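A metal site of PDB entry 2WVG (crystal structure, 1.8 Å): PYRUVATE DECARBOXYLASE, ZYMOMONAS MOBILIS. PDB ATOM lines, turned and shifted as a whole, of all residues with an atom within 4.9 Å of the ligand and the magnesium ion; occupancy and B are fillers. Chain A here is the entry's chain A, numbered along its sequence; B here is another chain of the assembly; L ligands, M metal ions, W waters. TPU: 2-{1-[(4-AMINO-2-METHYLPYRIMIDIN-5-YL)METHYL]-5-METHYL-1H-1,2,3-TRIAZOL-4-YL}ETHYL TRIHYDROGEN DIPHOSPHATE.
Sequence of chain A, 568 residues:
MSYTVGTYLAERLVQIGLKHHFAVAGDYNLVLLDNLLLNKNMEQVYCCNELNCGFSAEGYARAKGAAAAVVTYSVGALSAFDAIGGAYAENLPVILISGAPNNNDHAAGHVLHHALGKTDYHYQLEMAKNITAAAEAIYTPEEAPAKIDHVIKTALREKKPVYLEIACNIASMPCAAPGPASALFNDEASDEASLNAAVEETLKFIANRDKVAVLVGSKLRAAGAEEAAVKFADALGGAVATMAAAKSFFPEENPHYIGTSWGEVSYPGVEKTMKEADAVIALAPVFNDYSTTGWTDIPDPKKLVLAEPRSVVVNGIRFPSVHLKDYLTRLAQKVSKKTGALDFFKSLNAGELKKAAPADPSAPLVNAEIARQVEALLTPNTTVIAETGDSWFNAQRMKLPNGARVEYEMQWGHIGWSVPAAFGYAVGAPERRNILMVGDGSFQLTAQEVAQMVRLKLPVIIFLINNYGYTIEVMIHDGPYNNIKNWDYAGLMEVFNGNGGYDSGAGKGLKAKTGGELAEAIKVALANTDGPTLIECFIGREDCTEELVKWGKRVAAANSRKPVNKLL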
ATOM      1  N   THR A 388      10.299 -15.016  -8.774  1.00  0.00           N
ATOM      2  CA  THR A 388      10.683 -16.415  -8.681  1.00  0.00           C
ATOM      3  C   THR A 388      11.933 -16.538  -7.817  1.00  0.00           C
ATOM      4  O   THR A 388      12.917 -15.821  -8.030  1.00  0.00           O
ATOM      5  CB  THR A 388      11.006 -16.996 -10.061  1.00  0.00           C
ATOM      6  OG1 THR A 388       9.808 -17.044 -10.846  1.00  0.00           O
ATOM      7  CG2 THR A 388      11.562 -18.402  -9.943  1.00  0.00           C
ATOM      8  N   GLY A 389      11.887 -17.433  -6.839  1.00  0.00           N
ATOM      9  CA  GLY A 389      12.945 -17.541  -5.856  1.00  0.00           C
ATOM     10  C   GLY A 389      12.310 -17.759  -4.491  1.00  0.00           C
ATOM     11  O   GLY A 389      11.117 -18.068  -4.412  1.00  0.00           O
ATOM     12  N   ASP A 390      13.080 -17.622  -3.421  1.00  0.00           N
ATOM     13  CA  ASP A 390      12.460 -17.746  -2.101  1.00  0.00           C
ATOM     14  C   ASP A 390      11.389 -16.675  -1.855  1.00  0.00           C
ATOM     15  O   ASP A 390      10.515 -16.852  -1.006  1.00  0.00           O
ATOM     16  CB  ASP A 390      13.505 -17.740  -0.976  1.00  0.00           C
ATOM     17  CG  ASP A 390      12.966 -18.358   0.303  1.00  0.00           C
ATOM     18  OD1 ASP A 390      12.110 -19.259   0.206  1.00  0.00           O
ATOM     19  OD2 ASP A 390      13.388 -17.933   1.403  1.00  0.00           O
ATOM     20  N   SER A 391      11.455 -15.573  -2.602  1.00  0.00           N
ATOM     21  CA  SER A 391      10.423 -14.540  -2.502  1.00  0.00           C
ATOM     22  C   SER A 391       9.021 -15.077  -2.758  1.00  0.00           C
ATOM     23  O   SER A 391       8.048 -14.571  -2.196  1.00  0.00           O
ATOM     24  CB  SER A 391      10.735 -13.356  -3.422  1.00  0.00           C
ATOM     25  OG  SER A 391      11.863 -12.631  -2.947  1.00  0.00           O
ATOM     26  N   GLY A 413       7.608 -18.127 -15.048  1.00  0.00           N
ATOM     27  CA  GLY A 413       8.706 -18.208 -14.094  1.00  0.00           C
ATOM     28  C   GLY A 413      10.064 -17.760 -14.600  1.00  0.00           C
ATOM     29  O   GLY A 413      11.068 -18.399 -14.334  1.00  0.00           O
ATOM     30  N   HIS A 414      10.081 -16.649 -15.323  1.00  0.00           N
ATOM     31  CA  HIS A 414      11.304 -16.087 -15.885  1.00  0.00           C
ATOM     32  C   HIS A 414      11.958 -15.179 -14.854  1.00  0.00           C
ATOM     33  O   HIS A 414      11.433 -14.103 -14.561  1.00  0.00           O
ATOM     34  CB  HIS A 414      10.935 -15.273 -17.128  1.00  0.00           C
ATOM     35  CG  HIS A 414      12.110 -14.760 -17.910  1.00  0.00           C
ATOM     36  ND1 HIS A 414      13.041 -13.895 -17.387  1.00  0.00           N
ATOM     37  CD2 HIS A 414      12.477 -14.974 -19.193  1.00  0.00           C
ATOM     38  CE1 HIS A 414      13.950 -13.610 -18.296  1.00  0.00           C
ATOM     39  NE2 HIS A 414      13.632 -14.249 -19.408  1.00  0.00           N
ATOM     40  N   ILE A 415      13.099 -15.576 -14.284  1.00  0.00           N
ATOM     41  CA  ILE A 415      13.718 -14.706 -13.281  1.00  0.00           C
ATOM     42  C   ILE A 415      14.058 -13.376 -13.931  1.00  0.00           C
ATOM     43  O   ILE A 415      14.440 -13.341 -15.101  1.00  0.00           O
ATOM     44  CB  ILE A 415      14.952 -15.332 -12.560  1.00  0.00           C
ATOM     45  CG1 ILE A 415      16.061 -15.683 -13.546  1.00  0.00           C
ATOM     46  CG2 ILE A 415      14.537 -16.520 -11.691  1.00  0.00           C
ATOM     47  CD1 ILE A 415      17.376 -16.016 -12.840  1.00  0.00           C
ATOM     48  N   GLY A 439      15.108 -11.232  -5.577  1.00  0.00           N
ATOM     49  CA  GLY A 439      16.396 -11.801  -5.196  1.00  0.00           C
ATOM     50  C   GLY A 439      17.547 -11.201  -5.972  1.00  0.00           C
ATOM     51  O   GLY A 439      17.357 -10.678  -7.072  1.00  0.00           O
ATOM     52  N   ASP A 440      18.760 -11.297  -5.423  1.00  0.00           N
ATOM     53  CA  ASP A 440      19.944 -10.755  -6.098  1.00  0.00           C
ATOM     54  C   ASP A 440      20.172 -11.400  -7.476  1.00  0.00           C
ATOM     55  O   ASP A 440      20.543 -10.729  -8.444  1.00  0.00           O
ATOM     56  CB  ASP A 440      21.205 -10.880  -5.220  1.00  0.00           C
ATOM     57  CG  ASP A 440      21.505 -12.325  -4.806  1.00  0.00           C
ATOM     58  OD1 ASP A 440      20.571 -13.092  -4.528  1.00  0.00           O
ATOM     59  OD2 ASP A 440      22.698 -12.691  -4.740  1.00  0.00           O
ATOM     60  N   GLY A 441      19.948 -12.705  -7.576  1.00  0.00           N
ATOM     61  CA  GLY A 441      20.159 -13.405  -8.837  1.00  0.00           C
ATOM     62  C   GLY A 441      19.243 -12.911  -9.939  1.00  0.00           C
ATOM     63  O   GLY A 441      19.685 -12.649 -11.063  1.00  0.00           O
ATOM     64  N   SER A 442      17.957 -12.787  -9.616  1.00  0.00           N
ATOM     65  CA  SER A 442      16.950 -12.294 -10.557  1.00  0.00           C
ATOM     66  C   SER A 442      17.196 -10.837 -10.932  1.00  0.00           C
ATOM     67  O   SER A 442      17.053 -10.443 -12.085  1.00  0.00           O
ATOM     68  CB  SER A 442      15.551 -12.418  -9.959  1.00  0.00           C
ATOM     69  OG  SER A 442      15.207 -13.762  -9.700  1.00  0.00           O
ATOM     70  N   LEU A 445      19.380  -9.851 -13.986  1.00  0.00           N
ATOM     71  CA  LEU A 445      18.976 -10.070 -15.367  1.00  0.00           C
ATOM     72  C   LEU A 445      18.384  -8.831 -16.018  1.00  0.00           C
ATOM     73  O   LEU A 445      18.482  -8.658 -17.234  1.00  0.00           O
ATOM     74  CB  LEU A 445      17.969 -11.221 -15.491  1.00  0.00           C
ATOM     75  CG  LEU A 445      18.524 -12.641 -15.522  1.00  0.00           C
ATOM     76  CD1 LEU A 445      18.696 -13.144 -14.100  1.00  0.00           C
ATOM     77  CD2 LEU A 445      17.622 -13.578 -16.321  1.00  0.00           C
ATOM     78  N   ILE A 465      16.867  -8.924  -1.859  1.00  0.00           N
ATOM     79  CA  ILE A 465      17.326  -9.908  -0.894  1.00  0.00           C
ATOM     80  C   ILE A 465      18.673 -10.471  -1.346  1.00  0.00           C
ATOM     81  O   ILE A 465      18.747 -11.300  -2.244  1.00  0.00           O
ATOM     82  CB  ILE A 465      16.316 -11.059  -0.748  1.00  0.00           C
ATOM     83  CG1 ILE A 465      14.887 -10.508  -0.625  1.00  0.00           C
ATOM     84  CG2 ILE A 465      16.667 -11.927   0.450  1.00  0.00           C
ATOM     85  CD1 ILE A 465      14.687  -9.591   0.548  1.00  0.00           C
ATOM     86  N   ASN A 467      21.403 -12.783  -0.740  1.00  0.00           N
ATOM     87  CA  ASN A 467      21.958 -13.970  -0.091  1.00  0.00           C
ATOM     88  C   ASN A 467      23.065 -14.584  -0.936  1.00  0.00           C
ATOM     89  O   ASN A 467      23.410 -15.756  -0.785  1.00  0.00           O
ATOM     90  CB  ASN A 467      20.865 -14.995   0.209  1.00  0.00           C
ATOM     91  CG  ASN A 467      20.093 -15.421  -1.034  1.00  0.00           C
ATOM     92  OD1 ASN A 467      20.527 -15.145  -2.143  1.00  0.00           O
ATOM     93  ND2 ASN A 467      18.960 -16.089  -0.845  1.00  0.00           N
ATOM     94  N   TYR A 468      23.601 -13.773  -1.848  1.00  0.00           N
ATOM     95  CA  TYR A 468      24.803 -14.130  -2.613  1.00  0.00           C
ATOM     96  C   TYR A 468      24.646 -15.422  -3.433  1.00  0.00           C
ATOM     97  O   TYR A 468      25.400 -16.386  -3.250  1.00  0.00           O
ATOM     98  CB  TYR A 468      26.021 -14.197  -1.687  1.00  0.00           C
ATOM     99  CG  TYR A 468      27.370 -14.256  -2.386  1.00  0.00           C
ATOM    100  CD1 TYR A 468      27.596 -13.583  -3.579  1.00  0.00           C
ATOM    101  CD2 TYR A 468      28.415 -14.978  -1.836  1.00  0.00           C
ATOM    102  CE1 TYR A 468      28.839 -13.637  -4.215  1.00  0.00           C
ATOM    103  CE2 TYR A 468      29.659 -15.035  -2.444  1.00  0.00           C
ATOM    104  CZ  TYR A 468      29.866 -14.367  -3.629  1.00  0.00           C
ATOM    105  OH  TYR A 468      31.099 -14.444  -4.230  1.00  0.00           O
ATOM    106  N   GLY A 469      23.664 -15.453  -4.329  1.00  0.00           N
ATOM    107  CA  GLY A 469      23.504 -16.584  -5.224  1.00  0.00           C
ATOM    108  C   GLY A 469      22.079 -17.073  -5.427  1.00  0.00           C
ATOM    109  O   GLY A 469      21.130 -16.458  -4.938  1.00  0.00           O
ATOM    110  N   TYR A 470      21.942 -18.189  -6.124  1.00  0.00           N
ATOM    111  CA  TYR A 470      20.623 -18.719  -6.519  1.00  0.00           C
ATOM    112  C   TYR A 470      20.058 -19.725  -5.510  1.00  0.00           C
ATOM    113  O   TYR A 470      20.176 -20.937  -5.724  1.00  0.00           O
ATOM    114  CB  TYR A 470      20.726 -19.448  -7.860  1.00  0.00           C
ATOM    115  CG  TYR A 470      21.154 -18.634  -9.056  1.00  0.00           C
ATOM    116  CD1 TYR A 470      20.898 -17.274  -9.145  1.00  0.00           C
ATOM    117  CD2 TYR A 470      21.774 -19.262 -10.137  1.00  0.00           C
ATOM    118  CE1 TYR A 470      21.284 -16.553 -10.267  1.00  0.00           C
ATOM    119  CE2 TYR A 470      22.137 -18.568 -11.259  1.00  0.00           C
ATOM    120  CZ  TYR A 470      21.912 -17.219 -11.329  1.00  0.00           C
ATOM    121  OH  TYR A 470      22.292 -16.546 -12.474  1.00  0.00           O
ATOM    122  N   THR A 471      19.436 -19.259  -4.446  1.00  0.00           N
ATOM    123  CA  THR A 471      19.022 -20.174  -3.377  1.00  0.00           C
ATOM    124  C   THR A 471      17.936 -21.181  -3.807  1.00  0.00           C
ATOM    125  O   THR A 471      17.984 -22.342  -3.425  1.00  0.00           O
ATOM    126  CB  THR A 471      18.627 -19.397  -2.094  1.00  0.00           C
ATOM    127  OG1 THR A 471      19.810 -18.831  -1.526  1.00  0.00           O
ATOM    128  CG2 THR A 471      17.970 -20.311  -1.075  1.00  0.00           C
ATOM    129  N   ILE A 472      16.983 -20.757  -4.614  1.00  0.00           N
ATOM    130  CA  ILE A 472      15.981 -21.721  -5.039  1.00  0.00           C
ATOM    131  C   ILE A 472      16.587 -22.889  -5.853  1.00  0.00           C
ATOM    132  O   ILE A 472      16.123 -23.975  -5.727  1.00  0.00           O
ATOM    133  CB  ILE A 472      14.787 -21.069  -5.789  1.00  0.00           C
ATOM    134  CG1 ILE A 472      13.638 -22.057  -5.959  1.00  0.00           C
ATOM    135  CG2 ILE A 472      15.278 -20.390  -6.941  1.00  0.00           C
ATOM    136  CD1 ILE A 472      12.373 -21.511  -6.606  1.00  0.00           C
ATOM    137  N   GLU A 473      17.603 -22.604  -6.654  1.00  0.00           N
ATOM    138  CA  GLU A 473      18.283 -23.675  -7.374  1.00  0.00           C
ATOM    139  C   GLU A 473      19.132 -24.531  -6.438  1.00  0.00           C
ATOM    140  O   GLU A 473      19.222 -25.744  -6.608  1.00  0.00           O
ATOM    141  CB  GLU A 473      19.152 -23.085  -8.482  1.00  0.00           C
ATOM    142  CG  GLU A 473      18.400 -22.233  -9.480  1.00  0.00           C
ATOM    143  CD  GLU A 473      17.441 -23.056 -10.333  1.00  0.00           C
ATOM    144  OE1 GLU A 473      17.661 -23.126 -11.563  1.00  0.00           O
ATOM    145  OE2 GLU A 473      16.479 -23.630  -9.779  1.00  0.00           O
ATOM    146  N   VAL B  24      23.664 -20.536 -18.446  1.00  0.00           N
ATOM    147  CA  VAL B  24      22.825 -20.025 -17.367  1.00  0.00           C
ATOM    148  C   VAL B  24      22.010 -21.186 -16.807  1.00  0.00           C
ATOM    149  O   VAL B  24      21.264 -21.842 -17.527  1.00  0.00           O
ATOM    150  CB  VAL B  24      21.872 -18.923 -17.849  1.00  0.00           C
ATOM    151  CG1 VAL B  24      21.070 -18.401 -16.665  1.00  0.00           C
ATOM    152  CG2 VAL B  24      22.649 -17.790 -18.501  1.00  0.00           C
ATOM    153  N   ALA B  25      22.163 -21.441 -15.497  1.00  0.00           N
ATOM    154  CA  ALA B  25      21.487 -22.560 -14.858  1.00  0.00           C
ATOM    155  C   ALA B  25      19.970 -22.436 -14.841  1.00  0.00           C
ATOM    156  O   ALA B  25      19.417 -21.335 -14.701  1.00  0.00           O
ATOM    157  CB  ALA B  25      21.996 -22.713 -13.442  1.00  0.00           C
ATOM    158  N   GLY B  26      19.294 -23.577 -14.976  1.00  0.00           N
ATOM    159  CA  GLY B  26      17.853 -23.675 -14.771  1.00  0.00           C
ATOM    160  C   GLY B  26      17.552 -25.138 -14.479  1.00  0.00           C
ATOM    161  O   GLY B  26      18.349 -25.996 -14.853  1.00  0.00           O
ATOM    162  N   ASP B  27      16.434 -25.442 -13.836  1.00  0.00           N
ATOM    163  CA  ASP B  27      16.228 -26.828 -13.396  1.00  0.00           C
ATOM    164  C   ASP B  27      16.210 -27.872 -14.536  1.00  0.00           C
ATOM    165  O   ASP B  27      16.579 -29.034 -14.328  1.00  0.00           O
ATOM    166  CB  ASP B  27      15.063 -26.984 -12.394  1.00  0.00           C
ATOM    167  CG  ASP B  27      13.702 -26.668 -12.999  1.00  0.00           C
ATOM    168  OD1 ASP B  27      13.626 -26.089 -14.110  1.00  0.00           O
ATOM    169  OD2 ASP B  27      12.693 -27.010 -12.337  1.00  0.00           O
ATOM    170  N   GLU B  50      20.289 -14.853 -20.531  1.00  0.00           N
ATOM    171  CA  GLU B  50      20.464 -15.734 -21.679  1.00  0.00           C
ATOM    172  C   GLU B  50      20.758 -15.010 -22.980  1.00  0.00           C
ATOM    173  O   GLU B  50      21.459 -15.536 -23.839  1.00  0.00           O
ATOM    174  CB  GLU B  50      19.259 -16.675 -21.843  1.00  0.00           C
ATOM    175  CG  GLU B  50      19.154 -17.756 -20.773  1.00  0.00           C
ATOM    176  CD  GLU B  50      18.464 -17.297 -19.493  1.00  0.00           C
ATOM    177  OE1 GLU B  50      18.099 -16.104 -19.365  1.00  0.00           O
ATOM    178  OE2 GLU B  50      18.276 -18.148 -18.603  1.00  0.00           O
ATOM    179  N   THR B  72      18.139 -22.918 -20.284  1.00  0.00           N
ATOM    180  CA  THR B  72      17.011 -23.720 -19.855  1.00  0.00           C
ATOM    181  C   THR B  72      15.816 -23.589 -20.814  1.00  0.00           C
ATOM    182  O   THR B  72      15.727 -22.637 -21.597  1.00  0.00           O
ATOM    183  CB  THR B  72      16.593 -23.384 -18.406  1.00  0.00           C
ATOM    184  OG1 THR B  72      15.802 -24.467 -17.878  1.00  0.00           O
ATOM    185  CG2 THR B  72      15.799 -22.089 -18.354  1.00  0.00           C
ATOM    186  N   VAL B  75      11.990 -20.185 -21.121  1.00  0.00           N
ATOM    187  CA  VAL B  75      12.411 -18.899 -20.572  1.00  0.00           C
ATOM    188  C   VAL B  75      13.862 -18.574 -20.899  1.00  0.00           C
ATOM    189  O   VAL B  75      14.231 -17.409 -21.043  1.00  0.00           O
ATOM    190  CB  VAL B  75      12.191 -18.824 -19.037  1.00  0.00           C
ATOM    191  CG1 VAL B  75      10.705 -18.812 -18.709  1.00  0.00           C
ATOM    192  CG2 VAL B  75      12.894 -19.969 -18.322  1.00  0.00           C
ATOM    193  N   GLY B  76      14.704 -19.585 -21.008  1.00  0.00           N
ATOM    194  CA  GLY B  76      16.083 -19.351 -21.407  1.00  0.00           C
ATOM    195  C   GLY B  76      16.256 -19.281 -22.917  1.00  0.00           C
ATOM    196  O   GLY B  76      16.873 -18.354 -23.473  1.00  0.00           O
ATOM    197  N   HIS B 114       7.548 -23.115 -17.002  1.00  0.00           N
ATOM    198  CA  HIS B 114       8.354 -22.480 -18.046  1.00  0.00           C
ATOM    199  C   HIS B 114       7.718 -22.582 -19.435  1.00  0.00           C
ATOM    200  O   HIS B 114       8.249 -22.059 -20.399  1.00  0.00           O
ATOM    201  CB  HIS B 114       9.785 -23.034 -18.127  1.00  0.00           C
ATOM    202  CG  HIS B 114      10.647 -22.697 -16.950  1.00  0.00           C
ATOM    203  ND1 HIS B 114      10.345 -21.663 -16.083  1.00  0.00           N
ATOM    204  CD2 HIS B 114      11.810 -23.230 -16.517  1.00  0.00           C
ATOM    205  CE1 HIS B 114      11.283 -21.596 -15.147  1.00  0.00           C
ATOM    206  NE2 HIS B 114      12.182 -22.533 -15.397  1.00  0.00           N
HETATM  207  O23 TPU L   1      15.758 -15.989  -3.187  1.00  0.00           O
HETATM  208  P2  TPU L   1      16.645 -16.755  -4.327  1.00  0.00           P
HETATM  209  O22 TPU L   1      16.149 -18.307  -4.469  1.00  0.00           O
HETATM  210  O21 TPU L   1      18.065 -16.728  -3.982  1.00  0.00           O
HETATM  211  O11 TPU L   1      16.346 -15.951  -5.731  1.00  0.00           O
HETATM  212  P1  TPU L   1      17.434 -15.311  -6.763  1.00  0.00           P
HETATM  213  O12 TPU L   1      18.805 -14.684  -6.152  1.00  0.00           O
HETATM  214  O13 TPU L   1      16.702 -14.269  -7.503  1.00  0.00           O
HETATM  215  O5G TPU L   1      17.895 -16.528  -7.756  1.00  0.00           O
HETATM  216  C5B TPU L   1      16.933 -17.244  -8.488  1.00  0.00           C
HETATM  217  C5A TPU L   1      17.553 -18.447  -9.192  1.00  0.00           C
HETATM  218  C5  TPU L   1      16.733 -19.097 -10.297  1.00  0.00           C
HETATM  219  C4  TPU L   1      17.211 -19.494 -11.498  1.00  0.00           C
HETATM  220  C4A TPU L   1      18.636 -19.341 -12.032  1.00  0.00           C
HETATM  221  N1  TPU L   1      15.367 -19.421 -10.223  1.00  0.00           N
HETATM  222  N2  TPU L   1      15.051 -20.007 -11.382  1.00  0.00           N
HETATM  223  N3  TPU L   1      16.172 -20.057 -12.195  1.00  0.00           N
HETATM  224  C35 TPU L   1      16.255 -20.650 -13.534  1.00  0.00           C
HETATM  225  C5' TPU L   1      15.992 -19.617 -14.635  1.00  0.00           C
HETATM  226  C6' TPU L   1      16.958 -19.290 -15.494  1.00  0.00           C
HETATM  227  N1' TPU L   1      16.747 -18.354 -16.448  1.00  0.00           N
HETATM  228  C2' TPU L   1      15.493 -17.720 -16.529  1.00  0.00           C
HETATM  229  C2A TPU L   1      15.269 -16.623 -17.558  1.00  0.00           C
HETATM  230  N3' TPU L   1      14.490 -18.039 -15.632  1.00  0.00           N
HETATM  231  C4' TPU L   1      14.700 -18.951 -14.726  1.00  0.00           C
HETATM  232  N4' TPU L   1      13.634 -19.316 -13.821  1.00  0.00           N
HETATM  233 MG    MG M   1      19.603 -15.068  -4.164  1.00  0.00          MG
HETATM  234  O   HOH W   1      13.761 -14.310  -4.022  1.00  0.00           O
HETATM  235  O   HOH W   2      17.832 -13.786  -3.155  1.00  0.00           O
HETATM  236  O   HOH W   3      14.120 -13.818  -6.752  1.00  0.00           O
HETATM  237  O   HOH W   4      12.499 -21.996 -11.907  1.00  0.00           O
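An oxygen (O13) of the ligand is in hydrogen-bond range of the backbone NH (N) of Ser 442 (2.9 Å).
The backbone NH (N) of Ile 472 is in hydrogen-bond range of an oxygen (O22) of the ligand (2.6 Å).
The backbone NH (N) of Gly 441 lies close to an oxygen (O12) of the ligand.
A nitrogen (N3') of the ligand sits at hydrogen-bond distance from the backbone NH (N) of Ile 415 (3.1 Å).
An oxygen (O22) of the ligand lies within hydrogen-bond range of the backbone NH (N) of Thr 471, at 3.4 Å.
The backbone NH (N) of Asp 440 sits close to an oxygen (O12) of the ligand, 3.5 Å away.
A nitrogen (N1') of the ligand sits at hydrogen-bond distance from the side-chain carboxylate of Glu 50 of chain B (2.7 Å).
OG of Ser 442 is in hydrogen-bond range of O13 of the ligand.
The backbone carbonyl oxygen (O) of Gly 413 is in hydrogen-bond range of a nitrogen (N4') of the ligand (2.8 Å).
N of Asp 390 is in hydrogen-bond range of O23 of the ligand.
The side-chain amide nitrogen (ND2) of Asn 467 lies within hydrogen-bond range of the side-chain hydroxyl (OG1) of Thr 471.
N of Asp 440 lies within hydrogen-bond range of O of Ile 465, at 3.2 Å.
The side-chain carboxylate of Glu 473 sits at hydrogen-bond distance from the backbone NH of Asp 27 of chain B (3.5 Å).
The backbone NH (N) of Tyr 468 sits at hydrogen-bond distance from the side-chain carboxylate (OD2) of Asp 440 (3.2 Å).
The side-chain carboxylate (OE1) of Glu 473 lies close to a nitrogen (N3) of the ligand, at 3.5 Å.
Thr 388 touches the ligand (CG2 to N1, 3.9 Å).
Gly 389 touches the ligand.
His 414 touches the ligand.
Gly 439 touches the ligand.
Tyr 470 touches the ligand.
Ala 25 of chain B touches the ligand (O to C6', 3.3 Å).
CA of Gly 26 of chain B touches C35 of the ligand, at 3.6 Å.
CG2 of Val 75 of chain B touches N3' of the ligand, at 3.7 Å.
His 114 of chain B touches the ligand (CE1 to N4', 3.5 Å).
21 residues have an atom within 4 Å of the ligand: Thr 388, Gly 389, Asp 390, Gly 413, His 414, Ile 415, Gly 439, Asp 440, Gly 441, Ser 442, Asn 467, Gly 469, Tyr 470, Thr 471, Ile 472, Glu 473, Ala 25 of chain B, Gly 26 of chain B, Glu 50 of chain B, Val 75 of chain B and His 114 of chain B.
Of the 29 residues printed, 3 come within 4 Å of the magnesium ion.
Along chain A the residues within 4 Å of the magnesium ion span positions 440 to 469.
The nearest printed residue that does not touch the magnesium ion is Gly 441 (4.2 Å).
The magnesium ion is bound by O12 of the ligand (2.2 Å), O of Gly 469 (2.2 Å), OD1 of Asn 467 (2.2 Å), OD1 of Asp 440 (2.2 Å), O21 of the ligand (2.3 Å) and water W2 (2.4 Å).
Water W2 lies within hydrogen-bond range of O of Ile 465 (2.8 Å), O23 of the ligand (3.0 Å), ND2 of Asn 467 (3.5 Å) and N of Asp 440 (3.5 Å).
Water W3 lies within hydrogen-bond range of the backbone carbonyl oxygen of Thr 388 (2.7 Å), an oxygen (O13) of the ligand (2.7 Å), the backbone NH of Gly 439 (3.0 Å) and the side-chain hydroxyl of Ser 442 (3.1 Å).
Water W1 lies within hydrogen-bond range of an oxygen (O23) of the ligand (2.7 Å), the side-chain hydroxyl (OG) of Ser 391 (2.8 Å) and the backbone NH (N) of Asp 390 (3.4 Å).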
